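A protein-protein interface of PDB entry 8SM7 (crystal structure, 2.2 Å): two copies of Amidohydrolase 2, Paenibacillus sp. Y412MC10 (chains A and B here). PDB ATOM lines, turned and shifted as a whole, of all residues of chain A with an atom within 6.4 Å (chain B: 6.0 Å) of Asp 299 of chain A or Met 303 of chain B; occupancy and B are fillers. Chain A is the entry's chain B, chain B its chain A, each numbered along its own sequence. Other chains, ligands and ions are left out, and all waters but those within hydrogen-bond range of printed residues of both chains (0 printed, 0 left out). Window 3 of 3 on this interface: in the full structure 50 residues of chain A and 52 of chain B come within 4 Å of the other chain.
The side-chain amide nitrogen of Gln 295 of chain A sits at hydrogen-bond distance from the side-chain carboxylate of Asp 299 of chain A, 3.1 Å away.
Among the printed residues, pairs that only touch across the chains: Pro 291 of chain A with Trp 253 of chain B (3.6 Å), His 296 of chain A with Met 303 of chain B (3.6 Å), Asp 299 of chain A with Met 303 of chain B (3.7 Å), Leu 300 of chain A with Trp 253 of chain B (3.7 Å), Met 303 of chain A with Asp 299 of chain B (3.9 Å) and Met 303 of chain A with Met 303 of chain B (3.7 Å).
Of the printed residues of chain B, Pro 291 of chain A touches Trp 253 (3.6 Å).
Of the printed residues of chain B, His 296 of chain A touches Met 303.
Ile 298 of chain A touches none of the printed residues of chain B.
Of the printed residues of chain B, Met 303 of chain A touches Asp 299 and Met 303.
Of the printed residues of chain A, Trp 253 of chain B touches Pro 291 and Leu 300.
Of the printed residues of chain A, Asp 299 of chain B touches Met 303 (3.9 Å).
Phe 301 of chain B touches none of the printed residues of chain A.
Of chain A, only His 296, Asp 299 and Met 303 come within 4 Å of Met 303 of chain B.
The nearest residue of chain A that does not touch Met 303 of chain B is Leu 300 of chain A (4.2 Å).
Asp 299 of chain A touches Met 303 of chain B, and with the chains exchanged Met 303 of chain A touches Asp 299 of chain B.
Met 303 of chain B touches its own counterpart, Met 303 of chain A.
7 positions are printed for both chains.
Of the 6 pairs that touch across the chains among the printed residues, 3 have their exchanged pair printed and touching as well.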
ATOM      1  N   PRO A 291      30.101  26.515   4.297  1.00  0.00           N
ATOM      2  CA  PRO A 291      29.093  27.561   4.113  1.00  0.00           C
ATOM      3  C   PRO A 291      29.764  28.923   4.161  1.00  0.00           C
ATOM      4  O   PRO A 291      30.880  29.079   4.664  1.00  0.00           O
ATOM      5  CB  PRO A 291      28.142  27.376   5.301  1.00  0.00           C
ATOM      6  CG  PRO A 291      28.543  26.103   5.957  1.00  0.00           C
ATOM      7  CD  PRO A 291      29.951  25.805   5.575  1.00  0.00           C
ATOM      8  N   ASN A 293      28.682  31.389   5.983  1.00  0.00           N
ATOM      9  CA  ASN A 293      28.804  31.506   7.428  1.00  0.00           C
ATOM     10  C   ASN A 293      29.267  30.162   7.978  1.00  0.00           C
ATOM     11  O   ASN A 293      28.471  29.218   8.032  1.00  0.00           O
ATOM     12  CB  ASN A 293      27.480  31.918   8.050  1.00  0.00           C
ATOM     13  CG  ASN A 293      27.593  32.176   9.546  1.00  0.00           C
ATOM     14  OD1 ASN A 293      28.599  31.838  10.176  1.00  0.00           O
ATOM     15  ND2 ASN A 293      26.554  32.773  10.125  1.00  0.00           N
ATOM     16  N   PRO A 294      30.536  30.013   8.367  1.00  0.00           N
ATOM     17  CA  PRO A 294      30.989  28.711   8.886  1.00  0.00           C
ATOM     18  C   PRO A 294      30.198  28.236  10.083  1.00  0.00           C
ATOM     19  O   PRO A 294      30.138  27.021  10.338  1.00  0.00           O
ATOM     20  CB  PRO A 294      32.461  28.957   9.253  1.00  0.00           C
ATOM     21  CG  PRO A 294      32.696  30.442   9.065  1.00  0.00           C
ATOM     22  CD  PRO A 294      31.641  30.962   8.161  1.00  0.00           C
ATOM     23  N   GLN A 295      29.582  29.151  10.825  1.00  0.00           N
ATOM     24  CA  GLN A 295      28.734  28.726  11.928  1.00  0.00           C
ATOM     25  C   GLN A 295      27.638  27.775  11.462  1.00  0.00           C
ATOM     26  O   GLN A 295      27.226  26.886  12.224  1.00  0.00           O
ATOM     27  CB  GLN A 295      28.117  29.945  12.615  1.00  0.00           C
ATOM     28  CG  GLN A 295      27.333  29.612  13.873  1.00  0.00           C
ATOM     29  CD  GLN A 295      28.152  28.817  14.864  1.00  0.00           C
ATOM     30  OE1 GLN A 295      29.364  29.030  15.003  1.00  0.00           O
ATOM     31  NE2 GLN A 295      27.499  27.893  15.562  1.00  0.00           N
ATOM     32  N   HIS A 296      27.145  27.953  10.229  1.00  0.00           N
ATOM     33  CA  HIS A 296      26.009  27.159   9.766  1.00  0.00           C
ATOM     34  C   HIS A 296      26.328  25.663   9.801  1.00  0.00           C
ATOM     35  O   HIS A 296      25.538  24.855  10.311  1.00  0.00           O
ATOM     36  CB  HIS A 296      25.602  27.595   8.359  1.00  0.00           C
ATOM     37  CG  HIS A 296      24.946  28.941   8.306  1.00  0.00           C
ATOM     38  ND1 HIS A 296      24.464  29.580   9.429  1.00  0.00           N
ATOM     39  CD2 HIS A 296      24.687  29.768   7.263  1.00  0.00           C
ATOM     40  CE1 HIS A 296      23.937  30.741   9.080  1.00  0.00           C
ATOM     41  NE2 HIS A 296      24.058  30.879   7.772  1.00  0.00           N
ATOM     42  N   LEU A 297      27.488  25.272   9.265  1.00  0.00           N
ATOM     43  CA  LEU A 297      27.844  23.859   9.282  1.00  0.00           C
ATOM     44  C   LEU A 297      27.737  23.285  10.691  1.00  0.00           C
ATOM     45  O   LEU A 297      27.185  22.197  10.888  1.00  0.00           O
ATOM     46  CB  LEU A 297      29.247  23.666   8.717  1.00  0.00           C
ATOM     47  CG  LEU A 297      29.739  22.224   8.662  1.00  0.00           C
ATOM     48  CD1 LEU A 297      28.821  21.385   7.781  1.00  0.00           C
ATOM     49  CD2 LEU A 297      31.169  22.185   8.154  1.00  0.00           C
ATOM     50  N   ILE A 298      28.238  24.016  11.689  1.00  0.00           N
ATOM     51  CA  ILE A 298      28.172  23.544  13.069  1.00  0.00           C
ATOM     52  C   ILE A 298      26.728  23.466  13.543  1.00  0.00           C
ATOM     53  O   ILE A 298      26.337  22.502  14.215  1.00  0.00           O
ATOM     54  CB  ILE A 298      29.023  24.449  13.979  1.00  0.00           C
ATOM     55  CG1 ILE A 298      30.428  24.624  13.392  1.00  0.00           C
ATOM     56  CG2 ILE A 298      29.086  23.896  15.407  1.00  0.00           C
ATOM     57  CD1 ILE A 298      31.421  25.208  14.364  1.00  0.00           C
ATOM     58  N   ASP A 299      25.911  24.474  13.209  1.00  0.00           N
ATOM     59  CA  ASP A 299      24.481  24.403  13.507  1.00  0.00           C
ATOM     60  C   ASP A 299      23.868  23.130  12.933  1.00  0.00           C
ATOM     61  O   ASP A 299      23.000  22.507  13.556  1.00  0.00           O
ATOM     62  CB  ASP A 299      23.748  25.625  12.941  1.00  0.00           C
ATOM     63  CG  ASP A 299      24.130  26.935  13.633  1.00  0.00           C
ATOM     64  OD1 ASP A 299      24.728  26.910  14.732  1.00  0.00           O
ATOM     65  OD2 ASP A 299      23.818  28.006  13.063  1.00  0.00           O
ATOM     66  N   LEU A 300      24.311  22.730  11.741  1.00  0.00           N
ATOM     67  CA  LEU A 300      23.833  21.490  11.143  1.00  0.00           C
ATOM     68  C   LEU A 300      24.212  20.279  11.995  1.00  0.00           C
ATOM     69  O   LEU A 300      23.361  19.429  12.285  1.00  0.00           O
ATOM     70  CB  LEU A 300      24.383  21.357   9.722  1.00  0.00           C
ATOM     71  CG  LEU A 300      23.361  20.961   8.669  1.00  0.00           C
ATOM     72  CD1 LEU A 300      22.045  21.641   8.962  1.00  0.00           C
ATOM     73  CD2 LEU A 300      23.838  21.309   7.302  1.00  0.00           C
ATOM     74  N   PHE A 301      25.483  20.179  12.410  1.00  0.00           N
ATOM     75  CA  PHE A 301      25.886  19.068  13.280  1.00  0.00           C
ATOM     76  C   PHE A 301      24.970  18.957  14.485  1.00  0.00           C
ATOM     77  O   PHE A 301      24.526  17.863  14.850  1.00  0.00           O
ATOM     78  CB  PHE A 301      27.312  19.230  13.812  1.00  0.00           C
ATOM     79  CG  PHE A 301      28.359  19.293  12.767  1.00  0.00           C
ATOM     80  CD1 PHE A 301      28.082  18.946  11.455  1.00  0.00           C
ATOM     81  CD2 PHE A 301      29.622  19.750  13.090  1.00  0.00           C
ATOM     82  CE1 PHE A 301      29.062  19.029  10.485  1.00  0.00           C
ATOM     83  CE2 PHE A 301      30.608  19.827  12.141  1.00  0.00           C
ATOM     84  CZ  PHE A 301      30.332  19.468  10.828  1.00  0.00           C
ATOM     85  N   ASN A 302      24.728  20.086  15.152  1.00  0.00           N
ATOM     86  CA  ASN A 302      24.044  20.049  16.438  1.00  0.00           C
ATOM     87  C   ASN A 302      22.586  19.674  16.262  1.00  0.00           C
ATOM     88  O   ASN A 302      21.980  19.091  17.168  1.00  0.00           O
ATOM     89  CB  ASN A 302      24.188  21.400  17.141  1.00  0.00           C
ATOM     90  CG  ASN A 302      25.640  21.728  17.470  1.00  0.00           C
ATOM     91  OD1 ASN A 302      26.456  20.825  17.701  1.00  0.00           O
ATOM     92  ND2 ASN A 302      25.966  23.018  17.509  1.00  0.00           N
ATOM     93  N   MET A 303      22.035  19.948  15.100  1.00  0.00           N
ATOM     94  CA  MET A 303      20.653  19.607  14.826  1.00  0.00           C
ATOM     95  C   MET A 303      20.363  18.120  14.966  1.00  0.00           C
ATOM     96  O   MET A 303      19.239  17.743  15.235  1.00  0.00           O
ATOM     97  CB  MET A 303      20.310  20.041  13.412  1.00  0.00           C
ATOM     98  CG  MET A 303      19.953  21.494  13.241  1.00  0.00           C
ATOM     99  SD  MET A 303      19.475  21.778  11.533  1.00  0.00           S
ATOM    100  CE  MET A 303      19.808  23.527  11.398  1.00  0.00           C
ATOM    101  N   ILE A 304      21.371  17.282  14.770  1.00  0.00           N
ATOM    102  CA  ILE A 304      21.190  15.836  14.823  1.00  0.00           C
ATOM    103  C   ILE A 304      22.165  15.169  15.778  1.00  0.00           C
ATOM    104  O   ILE A 304      22.472  14.004  15.618  1.00  0.00           O
ATOM    105  CB  ILE A 304      21.338  15.224  13.416  1.00  0.00           C
ATOM    106  CG1 ILE A 304      22.670  15.620  12.791  1.00  0.00           C
ATOM    107  CG2 ILE A 304      20.196  15.658  12.515  1.00  0.00           C
ATOM    108  CD1 ILE A 304      23.067  14.740  11.631  1.00  0.00           C
ATOM    109  N   PRO B 249      21.285  22.573   0.861  1.00  0.00           N
ATOM    110  CA  PRO B 249      22.462  23.363   1.272  1.00  0.00           C
ATOM    111  C   PRO B 249      23.767  22.597   1.177  1.00  0.00           C
ATOM    112  O   PRO B 249      24.769  23.131   0.662  1.00  0.00           O
ATOM    113  CB  PRO B 249      22.133  23.748   2.719  1.00  0.00           C
ATOM    114  CG  PRO B 249      20.656  23.575   2.842  1.00  0.00           C
ATOM    115  CD  PRO B 249      20.333  22.406   1.971  1.00  0.00           C
ATOM    116  N   TRP B 253      26.927  23.751  -0.994  1.00  0.00           N
ATOM    117  CA  TRP B 253      28.267  23.954  -0.436  1.00  0.00           C
ATOM    118  C   TRP B 253      29.294  23.040  -1.098  1.00  0.00           C
ATOM    119  O   TRP B 253      30.406  23.475  -1.429  1.00  0.00           O
ATOM    120  CB  TRP B 253      28.255  23.743   1.074  1.00  0.00           C
ATOM    121  CG  TRP B 253      27.251  24.590   1.804  1.00  0.00           C
ATOM    122  CD1 TRP B 253      26.686  25.755   1.369  1.00  0.00           C
ATOM    123  CD2 TRP B 253      26.688  24.332   3.101  1.00  0.00           C
ATOM    124  NE1 TRP B 253      25.802  26.238   2.311  1.00  0.00           N
ATOM    125  CE2 TRP B 253      25.789  25.384   3.384  1.00  0.00           C
ATOM    126  CE3 TRP B 253      26.858  23.317   4.047  1.00  0.00           C
ATOM    127  CZ2 TRP B 253      25.061  25.445   4.575  1.00  0.00           C
ATOM    128  CZ3 TRP B 253      26.140  23.384   5.233  1.00  0.00           C
ATOM    129  CH2 TRP B 253      25.254  24.442   5.485  1.00  0.00           C
ATOM    130  N   ARG B 278      20.006  29.155  -7.092  1.00  0.00           N
ATOM    131  CA  ARG B 278      19.144  30.133  -6.432  1.00  0.00           C
ATOM    132  C   ARG B 278      18.349  30.950  -7.447  1.00  0.00           C
ATOM    133  O   ARG B 278      17.166  31.237  -7.227  1.00  0.00           O
ATOM    134  CB  ARG B 278      19.961  31.054  -5.519  1.00  0.00           C
ATOM    135  CG  ARG B 278      19.174  31.528  -4.269  1.00  0.00           C
ATOM    136  CD  ARG B 278      20.012  32.377  -3.301  1.00  0.00           C
ATOM    137  NE  ARG B 278      20.857  31.569  -2.428  1.00  0.00           N
ATOM    138  CZ  ARG B 278      22.174  31.463  -2.566  1.00  0.00           C
ATOM    139  NH1 ARG B 278      22.815  32.073  -3.555  1.00  0.00           N
ATOM    140  NH2 ARG B 278      22.862  30.711  -1.708  1.00  0.00           N
ATOM    141  N   ILE B 298      13.484  25.349   9.272  1.00  0.00           N
ATOM    142  CA  ILE B 298      13.478  26.759   8.894  1.00  0.00           C
ATOM    143  C   ILE B 298      14.880  27.341   9.000  1.00  0.00           C
ATOM    144  O   ILE B 298      15.346  28.049   8.096  1.00  0.00           O
ATOM    145  CB  ILE B 298      12.472  27.543   9.755  1.00  0.00           C
ATOM    146  CG1 ILE B 298      11.074  26.918   9.657  1.00  0.00           C
ATOM    147  CG2 ILE B 298      12.453  29.002   9.341  1.00  0.00           C
ATOM    148  CD1 ILE B 298      10.071  27.521  10.603  1.00  0.00           C
ATOM    149  N   ASP B 299      15.574  27.067  10.108  1.00  0.00           N
ATOM    150  CA  ASP B 299      16.984  27.433  10.196  1.00  0.00           C
ATOM    151  C   ASP B 299      17.723  26.972   8.955  1.00  0.00           C
ATOM    152  O   ASP B 299      18.572  27.690   8.411  1.00  0.00           O
ATOM    153  CB  ASP B 299      17.632  26.806  11.428  1.00  0.00           C
ATOM    154  CG  ASP B 299      17.032  27.291  12.720  1.00  0.00           C
ATOM    155  OD1 ASP B 299      16.123  28.152  12.692  1.00  0.00           O
ATOM    156  OD2 ASP B 299      17.480  26.791  13.769  1.00  0.00           O
ATOM    157  N   LEU B 300      17.403  25.769   8.487  1.00  0.00           N
ATOM    158  CA  LEU B 300      18.053  25.250   7.292  1.00  0.00           C
ATOM    159  C   LEU B 300      17.766  26.133   6.071  1.00  0.00           C
ATOM    160  O   LEU B 300      18.691  26.507   5.337  1.00  0.00           O
ATOM    161  CB  LEU B 300      17.608  23.809   7.072  1.00  0.00           C
ATOM    162  CG  LEU B 300      18.581  22.973   6.267  1.00  0.00           C
ATOM    163  CD1 LEU B 300      18.610  21.547   6.790  1.00  0.00           C
ATOM    164  CD2 LEU B 300      18.161  23.035   4.799  1.00  0.00           C
ATOM    165  N   PHE B 301      16.492  26.483   5.843  1.00  0.00           N
ATOM    166  CA  PHE B 301      16.133  27.375   4.736  1.00  0.00           C
ATOM    167  C   PHE B 301      16.985  28.638   4.737  1.00  0.00           C
ATOM    168  O   PHE B 301      17.551  29.029   3.708  1.00  0.00           O
ATOM    169  CB  PHE B 301      14.668  27.809   4.823  1.00  0.00           C
ATOM    170  CG  PHE B 301      13.678  26.717   4.656  1.00  0.00           C
ATOM    171  CD1 PHE B 301      14.069  25.436   4.322  1.00  0.00           C
ATOM    172  CD2 PHE B 301      12.325  26.985   4.842  1.00  0.00           C
ATOM    173  CE1 PHE B 301      13.125  24.433   4.181  1.00  0.00           C
ATOM    174  CE2 PHE B 301      11.373  25.998   4.702  1.00  0.00           C
ATOM    175  CZ  PHE B 301      11.770  24.719   4.370  1.00  0.00           C
ATOM    176  N   ASN B 302      17.034  29.322   5.884  1.00  0.00           N
ATOM    177  CA  ASN B 302      17.677  30.624   5.967  1.00  0.00           C
ATOM    178  C   ASN B 302      19.187  30.553   5.788  1.00  0.00           C
ATOM    179  O   ASN B 302      19.813  31.595   5.574  1.00  0.00           O
ATOM    180  CB  ASN B 302      17.330  31.287   7.300  1.00  0.00           C
ATOM    181  CG  ASN B 302      15.831  31.438   7.501  1.00  0.00           C
ATOM    182  OD1 ASN B 302      15.071  31.626   6.544  1.00  0.00           O
ATOM    183  ND2 ASN B 302      15.397  31.356   8.747  1.00  0.00           N
ATOM    184  N   MET B 303      19.768  29.381   5.892  1.00  0.00           N
ATOM    185  CA  MET B 303      21.191  29.250   5.684  1.00  0.00           C
ATOM    186  C   MET B 303      21.527  29.520   4.225  1.00  0.00           C
ATOM    187  O   MET B 303      22.603  29.996   3.912  1.00  0.00           O
ATOM    188  CB  MET B 303      21.645  27.858   6.085  1.00  0.00           C
ATOM    189  CG  MET B 303      21.663  27.571   7.566  1.00  0.00           C
ATOM    190  SD  MET B 303      22.267  25.902   7.850  1.00  0.00           S
ATOM    191  CE  MET B 303      22.115  25.799   9.626  1.00  0.00           C
ATOM    192  N   ILE B 304      20.592  29.247   3.337  1.00  0.00           N
ATOM    193  CA  ILE B 304      20.843  29.410   1.922  1.00  0.00           C
ATOM    194  C   ILE B 304      19.888  30.418   1.313  1.00  0.00           C
ATOM    195  O   ILE B 304      19.874  30.606   0.115  1.00  0.00           O
ATOM    196  CB  ILE B 304      20.720  28.049   1.238  1.00  0.00           C
ATOM    197  CG1 ILE B 304      19.348  27.441   1.492  1.00  0.00           C
ATOM    198  CG2 ILE B 304      21.797  27.113   1.748  1.00  0.00           C
ATOM    199  CD1 ILE B 304      19.068  26.236   0.627  1.00  0.00           C
ATOM    200  N   ASP B 305      19.115  31.087   2.146  1.00  0.00           N
ATOM    201  CA  ASP B 305      18.120  32.045   1.674  1.00  0.00           C
ATOM    202  C   ASP B 305      17.246  31.397   0.645  1.00  0.00           C
ATOM    203  O   ASP B 305      17.219  31.815  -0.503  1.00  0.00           O
ATOM    204  CB  ASP B 305      18.776  33.313   1.136  1.00  0.00           C
ATOM    205  CG  ASP B 305      17.919  34.528   1.340  1.00  0.00           C
ATOM    206  OD1 ASP B 305      16.964  34.453   2.141  1.00  0.00           O
ATOM    207  OD2 ASP B 305      18.194  35.559   0.698  1.00  0.00           O
ATOM    208  N   ALA B 306      16.491  30.400   1.062  1.00  0.00           N
ATOM    209  CA  ALA B 306      15.684  29.637   0.119  1.00  0.00           C
ATOM    210  C   ALA B 306      14.216  30.028   0.133  1.00  0.00           C
ATOM    211  O   ALA B 306      13.425  29.416  -0.585  1.00  0.00           O
ATOM    212  CB  ALA B 306      15.816  28.143   0.411  1.00  0.00           C
